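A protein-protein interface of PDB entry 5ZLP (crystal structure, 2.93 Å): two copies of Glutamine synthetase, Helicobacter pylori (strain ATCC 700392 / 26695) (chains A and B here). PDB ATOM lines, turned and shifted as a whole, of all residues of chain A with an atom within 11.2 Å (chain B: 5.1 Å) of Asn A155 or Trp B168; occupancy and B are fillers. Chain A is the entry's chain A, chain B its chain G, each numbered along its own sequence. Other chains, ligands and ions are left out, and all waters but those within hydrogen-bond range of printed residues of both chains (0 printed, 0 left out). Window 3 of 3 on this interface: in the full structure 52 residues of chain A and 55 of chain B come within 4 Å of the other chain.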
ATOM      1  N   LYS A 151      24.845  25.230 -25.601  1.00  0.00           N
ATOM      2  CA  LYS A 151      24.398  23.916 -25.157  1.00  0.00           C
ATOM      3  C   LYS A 151      24.803  23.716 -23.696  1.00  0.00           C
ATOM      4  O   LYS A 151      25.899  24.116 -23.298  1.00  0.00           O
ATOM      5  CB  LYS A 151      24.979  22.811 -26.053  1.00  0.00           C
ATOM      6  CG  LYS A 151      24.387  21.399 -25.820  1.00  0.00           C
ATOM      7  CD  LYS A 151      22.935  21.253 -26.274  1.00  0.00           C
ATOM      8  CE  LYS A 151      22.361  19.903 -25.847  1.00  0.00           C
ATOM      9  NZ  LYS A 151      20.956  19.696 -26.313  1.00  0.00           N
ATOM     10  N   ASP A 152      23.900  23.093 -22.879  1.00  0.00           N
ATOM     11  CA  ASP A 152      24.107  22.884 -21.423  1.00  0.00           C
ATOM     12  C   ASP A 152      23.715  21.441 -21.051  1.00  0.00           C
ATOM     13  O   ASP A 152      22.687  21.178 -20.417  1.00  0.00           O
ATOM     14  CB  ASP A 152      23.319  23.936 -20.621  1.00  0.00           C
ATOM     15  CG  ASP A 152      23.423  23.767 -19.108  1.00  0.00           C
ATOM     16  OD1 ASP A 152      24.313  23.052 -18.599  1.00  0.00           O
ATOM     17  OD2 ASP A 152      22.631  24.418 -18.396  1.00  0.00           O
ATOM     18  N   ALA A 153      24.583  20.496 -21.403  1.00  0.00           N
ATOM     19  CA  ALA A 153      24.343  19.072 -21.207  1.00  0.00           C
ATOM     20  C   ALA A 153      25.278  18.494 -20.153  1.00  0.00           C
ATOM     21  O   ALA A 153      26.175  19.156 -19.629  1.00  0.00           O
ATOM     22  CB  ALA A 153      24.509  18.300 -22.522  1.00  0.00           C
ATOM     23  N   SER A 154      25.036  17.226 -19.836  1.00  0.00           N
ATOM     24  CA  SER A 154      25.927  16.501 -18.949  1.00  0.00           C
ATOM     25  C   SER A 154      27.271  16.279 -19.617  1.00  0.00           C
ATOM     26  O   SER A 154      28.322  16.573 -19.041  1.00  0.00           O
ATOM     27  CB  SER A 154      25.295  15.167 -18.564  1.00  0.00           C
ATOM     28  OG  SER A 154      26.279  14.211 -18.163  1.00  0.00           O
ATOM     29  N   ASN A 155      27.246  15.800 -20.850  1.00  0.00           N
ATOM     30  CA  ASN A 155      28.435  15.405 -21.589  1.00  0.00           C
ATOM     31  C   ASN A 155      29.072  16.539 -22.386  1.00  0.00           C
ATOM     32  O   ASN A 155      30.032  16.280 -23.115  1.00  0.00           O
ATOM     33  CB  ASN A 155      28.093  14.245 -22.530  1.00  0.00           C
ATOM     34  CG  ASN A 155      27.140  14.648 -23.665  1.00  0.00           C
ATOM     35  OD1 ASN A 155      25.951  14.927 -23.461  1.00  0.00           O
ATOM     36  ND2 ASN A 155      27.664  14.640 -24.871  1.00  0.00           N
ATOM     37  N   SER A 156      28.598  17.785 -22.237  1.00  0.00           N
ATOM     38  CA  SER A 156      29.044  18.870 -23.106  1.00  0.00           C
ATOM     39  C   SER A 156      28.666  20.278 -22.635  1.00  0.00           C
ATOM     40  O   SER A 156      27.506  20.518 -22.292  1.00  0.00           O
ATOM     41  CB  SER A 156      28.469  18.615 -24.494  1.00  0.00           C
ATOM     42  OG  SER A 156      28.448  19.791 -25.265  1.00  0.00           O
ATOM     43  N   GLN A 157      29.619  21.228 -22.626  1.00  0.00           N
ATOM     44  CA  GLN A 157      29.321  22.658 -22.487  1.00  0.00           C
ATOM     45  C   GLN A 157      29.743  23.386 -23.756  1.00  0.00           C
ATOM     46  O   GLN A 157      30.788  23.089 -24.329  1.00  0.00           O
ATOM     47  CB  GLN A 157      30.023  23.310 -21.284  1.00  0.00           C
ATOM     48  CG  GLN A 157      29.821  22.623 -19.936  1.00  0.00           C
ATOM     49  CD  GLN A 157      28.372  22.470 -19.545  1.00  0.00           C
ATOM     50  OE1 GLN A 157      27.960  21.398 -19.091  1.00  0.00           O
ATOM     51  NE2 GLN A 157      27.591  23.536 -19.692  1.00  0.00           N
ATOM     52  N   TYR A 158      28.943  24.340 -24.211  1.00  0.00           N
ATOM     53  CA  TYR A 158      29.192  24.868 -25.546  1.00  0.00           C
ATOM     54  C   TYR A 158      28.533  26.221 -25.754  1.00  0.00           C
ATOM     55  O   TYR A 158      27.317  26.358 -25.587  1.00  0.00           O
ATOM     56  CB  TYR A 158      28.682  23.903 -26.604  1.00  0.00           C
ATOM     57  CG  TYR A 158      28.603  24.523 -27.984  1.00  0.00           C
ATOM     58  CD1 TYR A 158      29.765  24.838 -28.699  1.00  0.00           C
ATOM     59  CD2 TYR A 158      27.369  24.783 -28.586  1.00  0.00           C
ATOM     60  CE1 TYR A 158      29.702  25.384 -29.975  1.00  0.00           C
ATOM     61  CE2 TYR A 158      27.293  25.325 -29.856  1.00  0.00           C
ATOM     62  CZ  TYR A 158      28.462  25.626 -30.549  1.00  0.00           C
ATOM     63  OH  TYR A 158      28.392  26.177 -31.815  1.00  0.00           O
ATOM     64  N   SER A 468      30.546  24.111 -10.507  1.00  0.00           N
ATOM     65  CA  SER A 468      30.160  22.728 -10.612  1.00  0.00           C
ATOM     66  C   SER A 468      29.987  22.287 -12.046  1.00  0.00           C
ATOM     67  O   SER A 468      29.770  21.091 -12.284  1.00  0.00           O
ATOM     68  CB  SER A 468      28.857  22.488  -9.835  1.00  0.00           C
ATOM     69  OG  SER A 468      27.864  23.333 -10.362  1.00  0.00           O
ATOM     70  N   LYS A 469      30.082  23.206 -13.007  1.00  0.00           N
ATOM     71  CA  LYS A 469      29.946  22.827 -14.400  1.00  0.00           C
ATOM     72  C   LYS A 469      31.314  22.790 -15.042  1.00  0.00           C
ATOM     73  O   LYS A 469      31.993  23.828 -15.095  1.00  0.00           O
ATOM     74  CB  LYS A 469      29.031  23.782 -15.155  1.00  0.00           C
ATOM     75  CG  LYS A 469      27.574  23.355 -15.159  1.00  0.00           C
ATOM     76  CD  LYS A 469      26.706  24.512 -15.600  1.00  0.00           C
ATOM     77  CE  LYS A 469      25.282  24.296 -15.206  1.00  0.00           C
ATOM     78  NZ  LYS A 469      24.715  23.163 -15.967  1.00  0.00           N
ATOM     79  N   PRO A 470      31.745  21.625 -15.522  1.00  0.00           N
ATOM     80  CA  PRO A 470      33.032  21.513 -16.218  1.00  0.00           C
ATOM     81  C   PRO A 470      33.207  22.568 -17.300  1.00  0.00           C
ATOM     82  O   PRO A 470      32.316  22.794 -18.121  1.00  0.00           O
ATOM     83  CB  PRO A 470      32.980  20.106 -16.813  1.00  0.00           C
ATOM     84  CG  PRO A 470      32.079  19.372 -15.917  1.00  0.00           C
ATOM     85  CD  PRO A 470      31.073  20.325 -15.371  1.00  0.00           C
ATOM     86  N   HIS A 471      34.396  23.246 -17.278  1.00  0.00           N
ATOM     87  CA  HIS A 471      34.808  24.255 -18.251  1.00  0.00           C
ATOM     88  C   HIS A 471      35.516  23.585 -19.434  1.00  0.00           C
ATOM     89  O   HIS A 471      36.374  22.723 -19.221  1.00  0.00           O
ATOM     90  CB  HIS A 471      35.727  25.303 -17.605  1.00  0.00           C
ATOM     91  CG  HIS A 471      35.978  26.494 -18.482  1.00  0.00           C
ATOM     92  ND1 HIS A 471      36.773  26.435 -19.610  1.00  0.00           N
ATOM     93  CD2 HIS A 471      35.502  27.762 -18.426  1.00  0.00           C
ATOM     94  CE1 HIS A 471      36.783  27.613 -20.210  1.00  0.00           C
ATOM     95  NE2 HIS A 471      36.026  28.440 -19.508  1.00  0.00           N
ATOM     96  N   PRO A 472      35.144  23.897 -20.696  1.00  0.00           N
ATOM     97  CA  PRO A 472      35.915  23.395 -21.844  1.00  0.00           C
ATOM     98  C   PRO A 472      37.425  23.282 -21.631  1.00  0.00           C
ATOM     99  O   PRO A 472      37.989  22.203 -21.843  1.00  0.00           O
ATOM    100  CB  PRO A 472      35.559  24.408 -22.937  1.00  0.00           C
ATOM    101  CG  PRO A 472      34.104  24.793 -22.573  1.00  0.00           C
ATOM    102  CD  PRO A 472      33.824  24.374 -21.145  1.00  0.00           C
ATOM    103  N   PHE A 475      39.512  20.464 -20.113  1.00  0.00           N
ATOM    104  CA  PHE A 475      39.702  19.238 -20.883  1.00  0.00           C
ATOM    105  C   PHE A 475      41.010  19.270 -21.642  1.00  0.00           C
ATOM    106  O   PHE A 475      41.605  18.219 -21.891  1.00  0.00           O
ATOM    107  CB  PHE A 475      38.506  19.007 -21.811  1.00  0.00           C
ATOM    108  CG  PHE A 475      37.296  18.513 -21.081  1.00  0.00           C
ATOM    109  CD1 PHE A 475      36.543  19.377 -20.312  1.00  0.00           C
ATOM    110  CD2 PHE A 475      36.955  17.181 -21.104  1.00  0.00           C
ATOM    111  CE1 PHE A 475      35.454  18.911 -19.603  1.00  0.00           C
ATOM    112  CE2 PHE A 475      35.879  16.718 -20.412  1.00  0.00           C
ATOM    113  CZ  PHE A 475      35.131  17.571 -19.655  1.00  0.00           C
ATOM    114  N   TYR A 479      42.439  16.330 -19.244  1.00  0.00           N
ATOM    115  CA  TYR A 479      41.939  15.073 -19.788  1.00  0.00           C
ATOM    116  C   TYR A 479      42.987  13.967 -19.673  1.00  0.00           C
ATOM    117  O   TYR A 479      42.660  12.830 -19.338  1.00  0.00           O
ATOM    118  CB  TYR A 479      41.482  15.251 -21.226  1.00  0.00           C
ATOM    119  CG  TYR A 479      40.708  14.071 -21.772  1.00  0.00           C
ATOM    120  CD1 TYR A 479      39.383  13.833 -21.389  1.00  0.00           C
ATOM    121  CD2 TYR A 479      41.290  13.205 -22.707  1.00  0.00           C
ATOM    122  CE1 TYR A 479      38.667  12.760 -21.921  1.00  0.00           C
ATOM    123  CE2 TYR A 479      40.578  12.138 -23.251  1.00  0.00           C
ATOM    124  CZ  TYR A 479      39.276  11.912 -22.853  1.00  0.00           C
ATOM    125  OH  TYR A 479      38.599  10.832 -23.381  1.00  0.00           O
ATOM    126  N   TYR B 159      33.256  21.544 -25.454  1.00  0.00           N
ATOM    127  CA  TYR B 159      33.746  20.190 -25.267  1.00  0.00           C
ATOM    128  C   TYR B 159      32.562  19.247 -25.344  1.00  0.00           C
ATOM    129  O   TYR B 159      31.428  19.631 -25.047  1.00  0.00           O
ATOM    130  CB  TYR B 159      34.482  19.997 -23.940  1.00  0.00           C
ATOM    131  CG  TYR B 159      33.575  19.648 -22.791  1.00  0.00           C
ATOM    132  CD1 TYR B 159      33.024  20.645 -21.995  1.00  0.00           C
ATOM    133  CD2 TYR B 159      33.267  18.321 -22.488  1.00  0.00           C
ATOM    134  CE1 TYR B 159      32.205  20.350 -20.948  1.00  0.00           C
ATOM    135  CE2 TYR B 159      32.421  18.020 -21.423  1.00  0.00           C
ATOM    136  CZ  TYR B 159      31.904  19.049 -20.656  1.00  0.00           C
ATOM    137  OH  TYR B 159      31.066  18.781 -19.594  1.00  0.00           O
ATOM    138  N   GLU B 160      32.846  18.011 -25.744  1.00  0.00           N
ATOM    139  CA  GLU B 160      31.851  16.949 -25.754  1.00  0.00           C
ATOM    140  C   GLU B 160      32.590  15.626 -25.607  1.00  0.00           C
ATOM    141  O   GLU B 160      33.525  15.348 -26.362  1.00  0.00           O
ATOM    142  CB  GLU B 160      30.996  16.978 -27.043  1.00  0.00           C
ATOM    143  CG  GLU B 160      30.394  15.603 -27.459  1.00  0.00           C
ATOM    144  CD  GLU B 160      29.494  15.628 -28.687  1.00  0.00           C
ATOM    145  OE1 GLU B 160      28.860  14.572 -28.940  1.00  0.00           O
ATOM    146  OE2 GLU B 160      29.399  16.666 -29.403  1.00  0.00           O
ATOM    147  N   VAL B 161      32.199  14.844 -24.626  1.00  0.00           N
ATOM    148  CA  VAL B 161      32.620  13.446 -24.560  1.00  0.00           C
ATOM    149  C   VAL B 161      31.531  12.624 -25.236  1.00  0.00           C
ATOM    150  O   VAL B 161      30.368  13.043 -25.307  1.00  0.00           O
ATOM    151  CB  VAL B 161      32.863  12.986 -23.109  1.00  0.00           C
ATOM    152  CG1 VAL B 161      33.926  13.846 -22.404  1.00  0.00           C
ATOM    153  CG2 VAL B 161      31.583  13.009 -22.340  1.00  0.00           C
ATOM    154  N   ASP B 162      31.881  11.469 -25.775  1.00  0.00           N
ATOM    155  CA  ASP B 162      30.823  10.587 -26.236  1.00  0.00           C
ATOM    156  C   ASP B 162      31.135   9.162 -25.821  1.00  0.00           C
ATOM    157  O   ASP B 162      32.280   8.707 -25.907  1.00  0.00           O
ATOM    158  CB  ASP B 162      30.594  10.668 -27.751  1.00  0.00           C
ATOM    159  CG  ASP B 162      29.172  10.224 -28.155  1.00  0.00           C
ATOM    160  OD1 ASP B 162      28.332  10.058 -27.228  1.00  0.00           O
ATOM    161  OD2 ASP B 162      28.893  10.062 -29.382  1.00  0.00           O
ATOM    162  N   SER B 163      30.101   8.495 -25.320  1.00  0.00           N
ATOM    163  CA  SER B 163      30.050   7.065 -25.079  1.00  0.00           C
ATOM    164  C   SER B 163      28.667   6.605 -25.519  1.00  0.00           C
ATOM    165  O   SER B 163      27.713   7.387 -25.471  1.00  0.00           O
ATOM    166  CB  SER B 163      30.303   6.752 -23.593  1.00  0.00           C
ATOM    167  OG  SER B 163      30.463   5.365 -23.362  1.00  0.00           O
ATOM    168  N   GLY B 166      25.947   6.290 -22.707  1.00  0.00           N
ATOM    169  CA  GLY B 166      25.446   7.504 -22.107  1.00  0.00           C
ATOM    170  C   GLY B 166      24.018   7.818 -22.500  1.00  0.00           C
ATOM    171  O   GLY B 166      23.574   7.527 -23.600  1.00  0.00           O
ATOM    172  N   GLU B 167      23.308   8.473 -21.579  1.00  0.00           N
ATOM    173  CA  GLU B 167      21.905   8.836 -21.793  1.00  0.00           C
ATOM    174  C   GLU B 167      21.650   9.600 -23.083  1.00  0.00           C
ATOM    175  O   GLU B 167      20.548   9.539 -23.624  1.00  0.00           O
ATOM    176  CB  GLU B 167      21.409   9.686 -20.632  1.00  0.00           C
ATOM    177  CG  GLU B 167      21.080   8.865 -19.441  1.00  0.00           C
ATOM    178  CD  GLU B 167      20.353   9.658 -18.398  1.00  0.00           C
ATOM    179  OE1 GLU B 167      20.668  10.864 -18.289  1.00  0.00           O
ATOM    180  OE2 GLU B 167      19.492   9.080 -17.684  1.00  0.00           O
ATOM    181  N   TRP B 168      22.622  10.360 -23.566  1.00  0.00           N
ATOM    182  CA  TRP B 168      22.417  11.230 -24.710  1.00  0.00           C
ATOM    183  C   TRP B 168      22.385  10.475 -26.030  1.00  0.00           C
ATOM    184  O   TRP B 168      22.185  11.099 -27.085  1.00  0.00           O
ATOM    185  CB  TRP B 168      23.504  12.302 -24.726  1.00  0.00           C
ATOM    186  CG  TRP B 168      24.876  11.763 -24.628  1.00  0.00           C
ATOM    187  CD1 TRP B 168      25.711  11.489 -25.660  1.00  0.00           C
ATOM    188  CD2 TRP B 168      25.592  11.438 -23.438  1.00  0.00           C
ATOM    189  NE1 TRP B 168      26.906  11.003 -25.198  1.00  0.00           N
ATOM    190  CE2 TRP B 168      26.860  10.964 -23.829  1.00  0.00           C
ATOM    191  CE3 TRP B 168      25.286  11.496 -22.075  1.00  0.00           C
ATOM    192  CZ2 TRP B 168      27.832  10.550 -22.903  1.00  0.00           C
ATOM    193  CZ3 TRP B 168      26.254  11.093 -21.147  1.00  0.00           C
ATOM    194  CH2 TRP B 168      27.510  10.628 -21.569  1.00  0.00           C
ATOM    195  N   ASN B 169      22.549   9.156 -26.001  1.00  0.00           N
ATOM    196  CA  ASN B 169      22.537   8.361 -27.217  1.00  0.00           C
ATOM    197  C   ASN B 169      21.330   7.425 -27.323  1.00  0.00           C
ATOM    198  O   ASN B 169      21.277   6.599 -28.238  1.00  0.00           O
ATOM    199  CB  ASN B 169      23.854   7.595 -27.322  1.00  0.00           C
ATOM    200  CG  ASN B 169      24.976   8.472 -27.794  1.00  0.00           C
ATOM    201  OD1 ASN B 169      24.739   9.573 -28.269  1.00  0.00           O
ATOM    202  ND2 ASN B 169      26.197   7.993 -27.687  1.00  0.00           N
ATOM    203  N   ARG B 170      20.343   7.567 -26.440  1.00  0.00           N
ATOM    204  CA  ARG B 170      19.198   6.660 -26.434  1.00  0.00           C
ATOM    205  C   ARG B 170      18.465   6.667 -27.773  1.00  0.00           C
ATOM    206  O   ARG B 170      17.981   5.631 -28.233  1.00  0.00           O
ATOM    207  CB  ARG B 170      18.235   7.034 -25.297  1.00  0.00           C
ATOM    208  CG  ARG B 170      18.761   6.758 -23.903  1.00  0.00           C
ATOM    209  CD  ARG B 170      17.706   6.122 -23.012  1.00  0.00           C
ATOM    210  NE  ARG B 170      18.300   5.465 -21.851  1.00  0.00           N
ATOM    211  CZ  ARG B 170      18.429   6.027 -20.651  1.00  0.00           C
ATOM    212  NH1 ARG B 170      17.981   7.266 -20.435  1.00  0.00           N
ATOM    213  NH2 ARG B 170      18.994   5.338 -19.666  1.00  0.00           N
ATOM    214  N   ASP B 171      18.389   7.825 -28.413  1.00  0.00           N
ATOM    215  CA  ASP B 171      17.664   8.019 -29.655  1.00  0.00           C
ATOM    216  C   ASP B 171      18.565   7.943 -30.885  1.00  0.00           C
ATOM    217  O   ASP B 171      18.103   8.224 -31.997  1.00  0.00           O
ATOM    218  CB  ASP B 171      16.973   9.378 -29.609  1.00  0.00           C
ATOM    219  CG  ASP B 171      17.976  10.523 -29.391  1.00  0.00           C
ATOM    220  OD1 ASP B 171      18.996  10.284 -28.673  1.00  0.00           O
ATOM    221  OD2 ASP B 171      17.762  11.635 -29.952  1.00  0.00           O
ATOM    222  N   GLN B 226      28.487   6.656 -15.863  1.00  0.00           N
ATOM    223  CA  GLN B 226      28.079   5.928 -17.065  1.00  0.00           C
ATOM    224  C   GLN B 226      29.206   5.078 -17.640  1.00  0.00           C
ATOM    225  O   GLN B 226      29.107   3.846 -17.652  1.00  0.00           O
ATOM    226  CB  GLN B 226      27.492   6.897 -18.086  1.00  0.00           C
ATOM    227  CG  GLN B 226      26.292   7.570 -17.455  1.00  0.00           C
ATOM    228  CD  GLN B 226      25.579   8.603 -18.299  1.00  0.00           C
ATOM    229  OE1 GLN B 226      25.076   8.317 -19.372  1.00  0.00           O
ATOM    230  NE2 GLN B 226      25.504   9.817 -17.785  1.00  0.00           N
ATOM    231  N   LEU B 270      31.687  14.512 -16.586  1.00  0.00           N
ATOM    232  CA  LEU B 270      30.243  14.516 -16.834  1.00  0.00           C
ATOM    233  C   LEU B 270      29.551  15.274 -15.719  1.00  0.00           C
ATOM    234  O   LEU B 270      29.721  14.918 -14.545  1.00  0.00           O
ATOM    235  CB  LEU B 270      29.665  13.101 -16.894  1.00  0.00           C
ATOM    236  CG  LEU B 270      30.082  12.225 -18.052  1.00  0.00           C
ATOM    237  CD1 LEU B 270      29.535  10.869 -17.841  1.00  0.00           C
ATOM    238  CD2 LEU B 270      29.491  12.842 -19.239  1.00  0.00           C
ATOM    239  N   TYR B 271      28.767  16.303 -16.096  1.00  0.00           N
ATOM    240  CA  TYR B 271      27.906  17.010 -15.154  1.00  0.00           C
ATOM    241  C   TYR B 271      26.693  16.144 -14.836  1.00  0.00           C
ATOM    242  O   TYR B 271      26.078  15.565 -15.738  1.00  0.00           O
ATOM    243  CB  TYR B 271      27.472  18.366 -15.723  1.00  0.00           C
ATOM    244  CG  TYR B 271      26.705  19.262 -14.741  1.00  0.00           C
ATOM    245  CD1 TYR B 271      27.196  19.521 -13.471  1.00  0.00           C
ATOM    246  CD2 TYR B 271      25.506  19.861 -15.098  1.00  0.00           C
ATOM    247  CE1 TYR B 271      26.497  20.335 -12.568  1.00  0.00           C
ATOM    248  CE2 TYR B 271      24.805  20.671 -14.216  1.00  0.00           C
ATOM    249  CZ  TYR B 271      25.298  20.909 -12.942  1.00  0.00           C
ATOM    250  OH  TYR B 271      24.596  21.724 -12.047  1.00  0.00           O
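Of the printed residues of chain B, Ser A154 touches Tyr B159, Leu B270 and Tyr B271. Asn A155 touches five residues of chain B. Of the printed residues of chain B, Ser A468 touches Tyr B271 (3.2 Å). Printed residues of chain B within 4 Å of Phe A475: Tyr B159. Of chain A, only Ser A154, Asn A155, Ser A156, Gln A157, Pro A470, Pro A472 and Phe A475 come within 4 Å of Tyr B159. Of chain A, only Asn A155 and Ser A156 come within 4 Å of Glu B160. No residue of chain A comes within 4 Å of Ser B163. No residue of chain A comes within 4 Å of Gly B166. No residue of chain A comes within 4 Å of Glu B167. Of chain A, only Asn A155 (3.5 Å) comes within 4 Å of Trp B168. Asn B169 touches none of the printed residues of chain A. No residue of chain A comes within 4 Å of Asp B171. Leu B270 touches two residues of chain A. The nearest residue of chain A that does not touch Trp B168 is Ser A154 (4.3 Å). The nearest printed residue of chain A that does not touch Tyr B271 is Pro A470 (4.1 Å).
No position is printed for both chains. Of the 16 pairs that touch across the chains among the printed residues, none has its exchanged pair printed and touching as well.
Among the printed residues, merely in contact across the chains: Ser A154 with Tyr B159, Ser A154 with Leu B270, Asn A155 with Tyr B159, Asn A155 with Glu B160, Asn A155 with Trp B168, Asn A155 with Leu B270, Ser A156 with Glu B160, Ser A468 with Tyr B271, Lys A469 with Tyr B271, Pro A470 with Tyr B159, Pro A472 with Tyr B159 and Phe A475 with Tyr B159.
OD1 of Asp A152 lies within hydrogen-bond range of NE2 of Gln A157. The side-chain amino group (NZ) of Lys A469 lies within salt-bridge range of the side-chain carboxylate (OD1) of Asp A152 (2.7 Å). O of Ala A153 lies close to OE1 of Gln A157. OD1 of Asp B162 lies within hydrogen-bond range of NE1 of Trp B168 (2.7 Å).
OG of Ser A154 sits at hydrogen-bond distance from O of Tyr B271 (2.8 Å). The backbone carbonyl oxygen (O) of Asn A155 sits at hydrogen-bond distance from the backbone NH (N) of Val B161 (3.0 Å). The backbone carbonyl oxygen (O) of Tyr B159 lies within hydrogen-bond range of the side-chain hydroxyl (OG) of Ser A156 (3.0 Å). N of Tyr B159 sits at hydrogen-bond distance from O of Gln A157 (3.1 Å).
Of the 14 printed residues of chain B, 6 touch a printed residue of chain A. Hydrophobic or aromatic side chains of chain B within 4 Å of the printed part of chain A: Tyr B159, Val B161, Trp B168, Leu B270 and Tyr B271. Of the 15 printed residues of chain A, 9 touch a printed residue of chain B. Among the printed residues, no Asp or Glu carboxylate lies within 4 Å of a Lys or Arg side-chain nitrogen of the other chain.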
